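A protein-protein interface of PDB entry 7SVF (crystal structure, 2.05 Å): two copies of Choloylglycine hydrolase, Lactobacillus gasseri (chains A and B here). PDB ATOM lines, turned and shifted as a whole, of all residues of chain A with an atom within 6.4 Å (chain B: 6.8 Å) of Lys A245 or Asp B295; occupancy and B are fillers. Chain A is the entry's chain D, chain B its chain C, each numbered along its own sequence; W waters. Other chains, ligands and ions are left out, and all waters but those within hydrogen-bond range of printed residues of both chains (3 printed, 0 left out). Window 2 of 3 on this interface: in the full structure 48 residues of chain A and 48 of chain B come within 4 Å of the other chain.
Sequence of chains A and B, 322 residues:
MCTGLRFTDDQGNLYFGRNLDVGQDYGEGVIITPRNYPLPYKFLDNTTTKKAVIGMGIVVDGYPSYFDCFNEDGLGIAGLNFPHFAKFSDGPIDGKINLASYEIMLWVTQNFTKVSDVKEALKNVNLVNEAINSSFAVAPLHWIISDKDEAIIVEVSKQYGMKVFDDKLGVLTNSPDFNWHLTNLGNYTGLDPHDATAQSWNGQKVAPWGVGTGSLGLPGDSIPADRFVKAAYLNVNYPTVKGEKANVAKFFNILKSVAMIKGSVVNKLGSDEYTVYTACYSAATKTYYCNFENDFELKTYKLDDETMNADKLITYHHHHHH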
ATOM      1  N   TYR A  15     -22.750  34.444 -27.194  1.00  0.00           N
ATOM      2  CA  TYR A  15     -22.105  33.603 -28.193  1.00  0.00           C
ATOM      3  C   TYR A  15     -23.212  32.959 -29.018  1.00  0.00           C
ATOM      4  O   TYR A  15     -24.083  32.281 -28.462  1.00  0.00           O
ATOM      5  CB  TYR A  15     -21.194  32.565 -27.515  1.00  0.00           C
ATOM      6  CG  TYR A  15     -20.115  33.253 -26.704  1.00  0.00           C
ATOM      7  CD1 TYR A  15     -20.352  33.661 -25.397  1.00  0.00           C
ATOM      8  CD2 TYR A  15     -18.874  33.546 -27.272  1.00  0.00           C
ATOM      9  CE1 TYR A  15     -19.373  34.320 -24.663  1.00  0.00           C
ATOM     10  CE2 TYR A  15     -17.887  34.201 -26.550  1.00  0.00           C
ATOM     11  CZ  TYR A  15     -18.147  34.598 -25.253  1.00  0.00           C
ATOM     12  OH  TYR A  15     -17.168  35.255 -24.544  1.00  0.00           O
ATOM     13  N   LYS A 242     -16.395  30.535 -18.060  1.00  0.00           N
ATOM     14  CA  LYS A 242     -15.839  31.870 -17.874  1.00  0.00           C
ATOM     15  C   LYS A 242     -14.814  32.184 -18.957  1.00  0.00           C
ATOM     16  O   LYS A 242     -13.889  31.400 -19.190  1.00  0.00           O
ATOM     17  CB  LYS A 242     -15.197  31.994 -16.486  1.00  0.00           C
ATOM     18  N   GLY A 243     -14.978  33.327 -19.617  1.00  0.00           N
ATOM     19  CA  GLY A 243     -13.950  33.868 -20.486  1.00  0.00           C
ATOM     20  C   GLY A 243     -14.162  33.502 -21.949  1.00  0.00           C
ATOM     21  O   GLY A 243     -14.866  32.549 -22.292  1.00  0.00           O
ATOM     22  N   GLU A 244     -13.508  34.274 -22.826  1.00  0.00           N
ATOM     23  CA  GLU A 244     -13.748  34.172 -24.265  1.00  0.00           C
ATOM     24  C   GLU A 244     -13.343  32.809 -24.818  1.00  0.00           C
ATOM     25  O   GLU A 244     -14.115  32.169 -25.543  1.00  0.00           O
ATOM     26  CB  GLU A 244     -12.996  35.293 -24.990  1.00  0.00           C
ATOM     27  CG  GLU A 244     -13.056  35.227 -26.511  1.00  0.00           C
ATOM     28  CD  GLU A 244     -14.309  35.879 -27.105  1.00  0.00           C
ATOM     29  OE1 GLU A 244     -15.209  36.272 -26.340  1.00  0.00           O
ATOM     30  OE2 GLU A 244     -14.383  36.006 -28.346  1.00  0.00           O
ATOM     31  N   LYS A 245     -12.127  32.354 -24.507  1.00  0.00           N
ATOM     32  CA  LYS A 245     -11.654  31.070 -25.030  1.00  0.00           C
ATOM     33  C   LYS A 245     -12.562  29.916 -24.614  1.00  0.00           C
ATOM     34  O   LYS A 245     -12.914  29.064 -25.435  1.00  0.00           O
ATOM     35  CB  LYS A 245     -10.218  30.803 -24.564  1.00  0.00           C
ATOM     36  CG  LYS A 245      -9.161  31.538 -25.384  1.00  0.00           C
ATOM     37  CD  LYS A 245      -7.760  31.242 -24.853  1.00  0.00           C
ATOM     38  N   ALA A 246     -12.930  29.852 -23.334  1.00  0.00           N
ATOM     39  CA  ALA A 246     -13.750  28.734 -22.871  1.00  0.00           C
ATOM     40  C   ALA A 246     -15.153  28.784 -23.473  1.00  0.00           C
ATOM     41  O   ALA A 246     -15.738  27.741 -23.786  1.00  0.00           O
ATOM     42  CB  ALA A 246     -13.821  28.723 -21.342  1.00  0.00           C
ATOM     43  N   ASN A 247     -15.714  29.986 -23.644  1.00  0.00           N
ATOM     44  CA  ASN A 247     -17.070  30.082 -24.177  1.00  0.00           C
ATOM     45  C   ASN A 247     -17.106  29.741 -25.660  1.00  0.00           C
ATOM     46  O   ASN A 247     -18.009  29.026 -26.115  1.00  0.00           O
ATOM     47  CB  ASN A 247     -17.631  31.479 -23.918  1.00  0.00           C
ATOM     48  CG  ASN A 247     -18.280  31.578 -22.563  1.00  0.00           C
ATOM     49  OD1 ASN A 247     -19.430  31.179 -22.388  1.00  0.00           O
ATOM     50  ND2 ASN A 247     -17.538  32.081 -21.585  1.00  0.00           N
ATOM     51  N   VAL A 248     -16.117  30.213 -26.426  1.00  0.00           N
ATOM     52  CA  VAL A 248     -16.013  29.836 -27.832  1.00  0.00           C
ATOM     53  C   VAL A 248     -15.812  28.331 -27.966  1.00  0.00           C
ATOM     54  O   VAL A 248     -16.374  27.692 -28.865  1.00  0.00           O
ATOM     55  CB  VAL A 248     -14.876  30.624 -28.517  1.00  0.00           C
ATOM     56  CG1 VAL A 248     -14.572  30.034 -29.888  1.00  0.00           C
ATOM     57  CG2 VAL A 248     -15.249  32.108 -28.654  1.00  0.00           C
ATOM     58  N   ALA A 249     -14.987  27.741 -27.091  1.00  0.00           N
ATOM     59  CA  ALA A 249     -14.764  26.300 -27.157  1.00  0.00           C
ATOM     60  C   ALA A 249     -16.036  25.539 -26.809  1.00  0.00           C
ATOM     61  O   ALA A 249     -16.417  24.597 -27.512  1.00  0.00           O
ATOM     62  CB  ALA A 249     -13.615  25.894 -26.226  1.00  0.00           C
ATOM     63  N   LYS A 250     -16.705  25.935 -25.723  1.00  0.00           N
ATOM     64  CA  LYS A 250     -18.008  25.354 -25.400  1.00  0.00           C
ATOM     65  C   LYS A 250     -18.936  25.426 -26.602  1.00  0.00           C
ATOM     66  O   LYS A 250     -19.644  24.464 -26.904  1.00  0.00           O
ATOM     67  CB  LYS A 250     -18.633  26.079 -24.198  1.00  0.00           C
ATOM     68  CG  LYS A 250     -20.165  25.986 -24.095  1.00  0.00           C
ATOM     69  CD  LYS A 250     -20.706  26.739 -22.868  1.00  0.00           C
ATOM     70  CE  LYS A 250     -22.253  26.787 -22.871  1.00  0.00           C
ATOM     71  NZ  LYS A 250     -22.834  27.262 -21.585  1.00  0.00           N
ATOM     72  N   ASN A 253     -17.818  22.925 -29.144  1.00  0.00           N
ATOM     73  CA  ASN A 253     -18.050  21.580 -28.607  1.00  0.00           C
ATOM     74  C   ASN A 253     -19.482  21.120 -28.881  1.00  0.00           C
ATOM     75  O   ASN A 253     -19.710  19.984 -29.315  1.00  0.00           O
ATOM     76  CB  ASN A 253     -17.759  21.547 -27.100  1.00  0.00           C
ATOM     77  CG  ASN A 253     -16.263  21.719 -26.773  1.00  0.00           C
ATOM     78  OD1 ASN A 253     -15.396  21.444 -27.608  1.00  0.00           O
ATOM     79  ND2 ASN A 253     -15.966  22.181 -25.552  1.00  0.00           N
ATOM     80  N   TYR A 289     -15.726  33.757 -35.414  1.00  0.00           N
ATOM     81  CA  TYR A 289     -14.878  32.566 -35.514  1.00  0.00           C
ATOM     82  C   TYR A 289     -15.529  31.544 -36.434  1.00  0.00           C
ATOM     83  O   TYR A 289     -16.754  31.374 -36.419  1.00  0.00           O
ATOM     84  CB  TYR A 289     -14.677  31.896 -34.158  1.00  0.00           C
ATOM     85  CG  TYR A 289     -14.137  32.739 -33.035  1.00  0.00           C
ATOM     86  CD1 TYR A 289     -14.921  33.700 -32.403  1.00  0.00           C
ATOM     87  CD2 TYR A 289     -12.842  32.542 -32.582  1.00  0.00           C
ATOM     88  CE1 TYR A 289     -14.411  34.453 -31.350  1.00  0.00           C
ATOM     89  CE2 TYR A 289     -12.326  33.283 -31.546  1.00  0.00           C
ATOM     90  CZ  TYR A 289     -13.100  34.232 -30.933  1.00  0.00           C
ATOM     91  OH  TYR A 289     -12.546  34.949 -29.897  1.00  0.00           O
ATOM     92  N   CYS B 290      -3.736  19.012 -31.368  1.00  0.00           N
ATOM     93  CA  CYS B 290      -4.756  18.783 -30.346  1.00  0.00           C
ATOM     94  C   CYS B 290      -5.517  20.066 -30.029  1.00  0.00           C
ATOM     95  O   CYS B 290      -5.026  21.175 -30.251  1.00  0.00           O
ATOM     96  CB  CYS B 290      -4.120  18.230 -29.060  1.00  0.00           C
ATOM     97  SG  CYS B 290      -2.808  19.340 -28.520  1.00  0.00           S
ATOM     98  N   ASN B 291      -6.723  19.899 -29.483  1.00  0.00           N
ATOM     99  CA  ASN B 291      -7.426  21.002 -28.854  1.00  0.00           C
ATOM    100  C   ASN B 291      -8.084  20.469 -27.591  1.00  0.00           C
ATOM    101  O   ASN B 291      -8.042  19.269 -27.297  1.00  0.00           O
ATOM    102  CB  ASN B 291      -8.418  21.700 -29.822  1.00  0.00           C
ATOM    103  CG  ASN B 291      -9.701  20.909 -30.074  1.00  0.00           C
ATOM    104  OD1 ASN B 291      -9.914  19.801 -29.545  1.00  0.00           O
ATOM    105  ND2 ASN B 291     -10.591  21.505 -30.886  1.00  0.00           N
ATOM    106  N   PHE B 292      -8.664  21.382 -26.821  1.00  0.00           N
ATOM    107  CA  PHE B 292      -9.106  21.091 -25.469  1.00  0.00           C
ATOM    108  C   PHE B 292     -10.545  21.551 -25.282  1.00  0.00           C
ATOM    109  O   PHE B 292     -11.065  22.355 -26.059  1.00  0.00           O
ATOM    110  CB  PHE B 292      -8.188  21.766 -24.461  1.00  0.00           C
ATOM    111  CG  PHE B 292      -6.793  21.213 -24.480  1.00  0.00           C
ATOM    112  CD1 PHE B 292      -5.870  21.675 -25.406  1.00  0.00           C
ATOM    113  CD2 PHE B 292      -6.426  20.206 -23.611  1.00  0.00           C
ATOM    114  CE1 PHE B 292      -4.579  21.143 -25.448  1.00  0.00           C
ATOM    115  CE2 PHE B 292      -5.132  19.672 -23.639  1.00  0.00           C
ATOM    116  CZ  PHE B 292      -4.220  20.145 -24.563  1.00  0.00           C
ATOM    117  N   GLU B 293     -11.167  21.037 -24.219  1.00  0.00           N
ATOM    118  CA  GLU B 293     -12.553  21.385 -23.922  1.00  0.00           C
ATOM    119  C   GLU B 293     -12.740  22.886 -23.729  1.00  0.00           C
ATOM    120  O   GLU B 293     -13.803  23.424 -24.066  1.00  0.00           O
ATOM    121  CB  GLU B 293     -13.022  20.648 -22.669  1.00  0.00           C
ATOM    122  CG  GLU B 293     -14.503  20.867 -22.339  1.00  0.00           C
ATOM    123  CD  GLU B 293     -14.743  22.105 -21.472  1.00  0.00           C
ATOM    124  OE1 GLU B 293     -13.844  22.461 -20.667  1.00  0.00           O
ATOM    125  OE2 GLU B 293     -15.833  22.720 -21.593  1.00  0.00           O
ATOM    126  N   ASN B 294     -11.741  23.569 -23.162  1.00  0.00           N
ATOM    127  CA  ASN B 294     -11.835  24.993 -22.861  1.00  0.00           C
ATOM    128  C   ASN B 294     -10.971  25.841 -23.789  1.00  0.00           C
ATOM    129  O   ASN B 294     -10.730  27.021 -23.505  1.00  0.00           O
ATOM    130  CB  ASN B 294     -11.465  25.264 -21.400  1.00  0.00           C
ATOM    131  CG  ASN B 294     -10.001  24.958 -21.101  1.00  0.00           C
ATOM    132  OD1 ASN B 294      -9.278  24.436 -21.947  1.00  0.00           O
ATOM    133  ND2 ASN B 294      -9.563  25.284 -19.895  1.00  0.00           N
ATOM    134  N   ASP B 295     -10.517  25.277 -24.908  1.00  0.00           N
ATOM    135  CA  ASP B 295      -9.711  26.047 -25.863  1.00  0.00           C
ATOM    136  C   ASP B 295      -9.714  25.290 -27.189  1.00  0.00           C
ATOM    137  O   ASP B 295      -8.951  24.331 -27.358  1.00  0.00           O
ATOM    138  CB  ASP B 295      -8.295  26.267 -25.357  1.00  0.00           C
ATOM    139  CG  ASP B 295      -7.487  27.189 -26.278  1.00  0.00           C
ATOM    140  OD1 ASP B 295      -7.930  27.441 -27.420  1.00  0.00           O
ATOM    141  OD2 ASP B 295      -6.408  27.652 -25.871  1.00  0.00           O
ATOM    142  N   PHE B 296     -10.542  25.754 -28.123  1.00  0.00           N
ATOM    143  CA  PHE B 296     -10.806  24.999 -29.338  1.00  0.00           C
ATOM    144  C   PHE B 296      -9.732  25.163 -30.415  1.00  0.00           C
ATOM    145  O   PHE B 296      -9.719  24.380 -31.372  1.00  0.00           O
ATOM    146  CB  PHE B 296     -12.177  25.396 -29.902  1.00  0.00           C
ATOM    147  CG  PHE B 296     -12.870  24.279 -30.616  1.00  0.00           C
ATOM    148  CD1 PHE B 296     -13.545  23.298 -29.901  1.00  0.00           C
ATOM    149  CD2 PHE B 296     -12.841  24.201 -31.999  1.00  0.00           C
ATOM    150  CE1 PHE B 296     -14.166  22.262 -30.549  1.00  0.00           C
ATOM    151  CE2 PHE B 296     -13.458  23.167 -32.655  1.00  0.00           C
ATOM    152  CZ  PHE B 296     -14.129  22.193 -31.930  1.00  0.00           C
ATOM    153  N   GLU B 297      -8.835  26.140 -30.297  1.00  0.00           N
ATOM    154  CA  GLU B 297      -7.833  26.333 -31.342  1.00  0.00           C
ATOM    155  C   GLU B 297      -6.901  25.131 -31.413  1.00  0.00           C
ATOM    156  O   GLU B 297      -6.401  24.660 -30.387  1.00  0.00           O
ATOM    157  CB  GLU B 297      -7.025  27.605 -31.096  1.00  0.00           C
ATOM    158  CG  GLU B 297      -6.056  27.931 -32.234  1.00  0.00           C
ATOM    159  CD  GLU B 297      -6.759  28.041 -33.581  1.00  0.00           C
ATOM    160  OE1 GLU B 297      -6.758  27.054 -34.375  1.00  0.00           O
ATOM    161  OE2 GLU B 297      -7.317  29.130 -33.847  1.00  0.00           O
ATOM    162  N   LEU B 298      -6.683  24.633 -32.632  1.00  0.00           N
ATOM    163  CA  LEU B 298      -5.767  23.520 -32.850  1.00  0.00           C
ATOM    164  C   LEU B 298      -4.345  23.949 -32.515  1.00  0.00           C
ATOM    165  O   LEU B 298      -3.844  24.935 -33.064  1.00  0.00           O
ATOM    166  CB  LEU B 298      -5.821  23.059 -34.306  1.00  0.00           C
ATOM    167  CG  LEU B 298      -6.887  22.081 -34.760  1.00  0.00           C
ATOM    168  CD1 LEU B 298      -6.426  21.349 -36.013  1.00  0.00           C
ATOM    169  CD2 LEU B 298      -7.249  21.104 -33.643  1.00  0.00           C
ATOM    170  N   LYS B 299      -3.688  23.215 -31.621  1.00  0.00           N
ATOM    171  CA  LYS B 299      -2.268  23.422 -31.350  1.00  0.00           C
ATOM    172  C   LYS B 299      -1.457  22.318 -32.012  1.00  0.00           C
ATOM    173  O   LYS B 299      -1.904  21.170 -32.082  1.00  0.00           O
ATOM    174  CB  LYS B 299      -1.975  23.432 -29.851  1.00  0.00           C
ATOM    175  CG  LYS B 299      -3.070  24.023 -29.022  1.00  0.00           C
ATOM    176  CD  LYS B 299      -2.660  25.312 -28.357  1.00  0.00           C
ATOM    177  CE  LYS B 299      -3.572  25.577 -27.154  1.00  0.00           C
ATOM    178  NZ  LYS B 299      -3.290  26.891 -26.526  1.00  0.00           N
HETATM  179  O   HOH W   1     -12.791  20.764 -27.606  1.00  0.00           O
HETATM  180  O   HOH W   2     -11.734  28.383 -27.919  1.00  0.00           O
HETATM  181  O   HOH W   3     -15.337  25.453 -22.083  1.00  0.00           O
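ND2 of Asn A253 lies within hydrogen-bond range of O of Glu B293 (2.9 Å).
The side-chain amide nitrogen of Asn B291 sits at hydrogen-bond distance from the backbone carbonyl oxygen of Phe B296 (3.0 Å). The backbone NH (N) of Glu B297 sits at hydrogen-bond distance from the side-chain carboxylate (OD1) of Asp B295 (3.3 Å). NZ of Lys B299 is in salt-bridge range of OD2 of Asp B295, at 3.3 Å. The side-chain amide nitrogen of Asn A253 lies close to the backbone carbonyl oxygen of Ala A249 (3.1 Å).
Asn B294 touches Lys A245 (O to O, 3.6 Å). OD2 of Asp B295 touches CD of Lys A245 (3.97 Å). CA of Ala A246 touches O of Asn B294, 3.5 Å away. Ala A249 touches Glu B293. Ala A249 touches Asn B294. Asp B295 touches Ala A249. Ala A249 touches Phe B296. Asn A253 touches Phe B296 (OD1 to CE1, 3.3 Å).
Lys A245 touches just these residues of chain B: Asn B294 (3.6 Å) and Asp B295 (3.97 Å). Printed residues of chain B within 4 Å of Ala A249: Glu B293, Asn B294, Asp B295 and Phe B296. Printed residues of chain B within 4 Å of Asn A253: Glu B293 (2.9 Å) and Phe B296 (3.3 Å). Printed residues of chain A within 4 Å of Glu B293: Ala A249 (3.3 Å) and Asn A253 (2.9 Å). Asp B295 touches just these residues of chain A: Lys A245 (3.97 Å) and Ala A249 (3.4 Å). Printed residues of chain A within 4 Å of Phe B296: Ala A249 (3.6 Å) and Asn A253 (3.3 Å). The nearest residue of chain B that does not touch Lys A245 is Phe B296 (4.9 Å). The nearest printed residue of chain B that does not touch Ala A246 is Glu B293 (4.7 Å).
Of the 12 printed residues of chain A, 4 touch a printed residue of chain B. Printed residues of chain A that touch a printed residue of chain B: Lys A245, Ala A246, Ala A249 and Asn A253. Hydrophobic or aromatic side chains of chain A that line the printed part of chain B: Ala A249. Among the printed residues, 9 pairs touch across the chains.
No position is printed for both chains. Of the 9 pairs that touch across the chains among the printed residues, none has its exchanged pair printed and touching as well.
Water W1 lies within hydrogen-bond range of the side-chain amide oxygen of Asn A253 (2.7 Å) and the backbone carbonyl oxygen of Phe B292 (2.8 Å). Water W3 lies within hydrogen-bond range of the side-chain carboxylate (OE2) of Glu B293 (2.8 Å) and the backbone carbonyl oxygen (O) of Ala A246 (2.9 Å). Water W2 lies within hydrogen-bond range of the backbone carbonyl oxygen (O) of Lys A245 (2.8 Å), the backbone NH (N) of Phe B296 (2.9 Å) and the backbone NH (N) of Ala A249 (3.4 Å).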
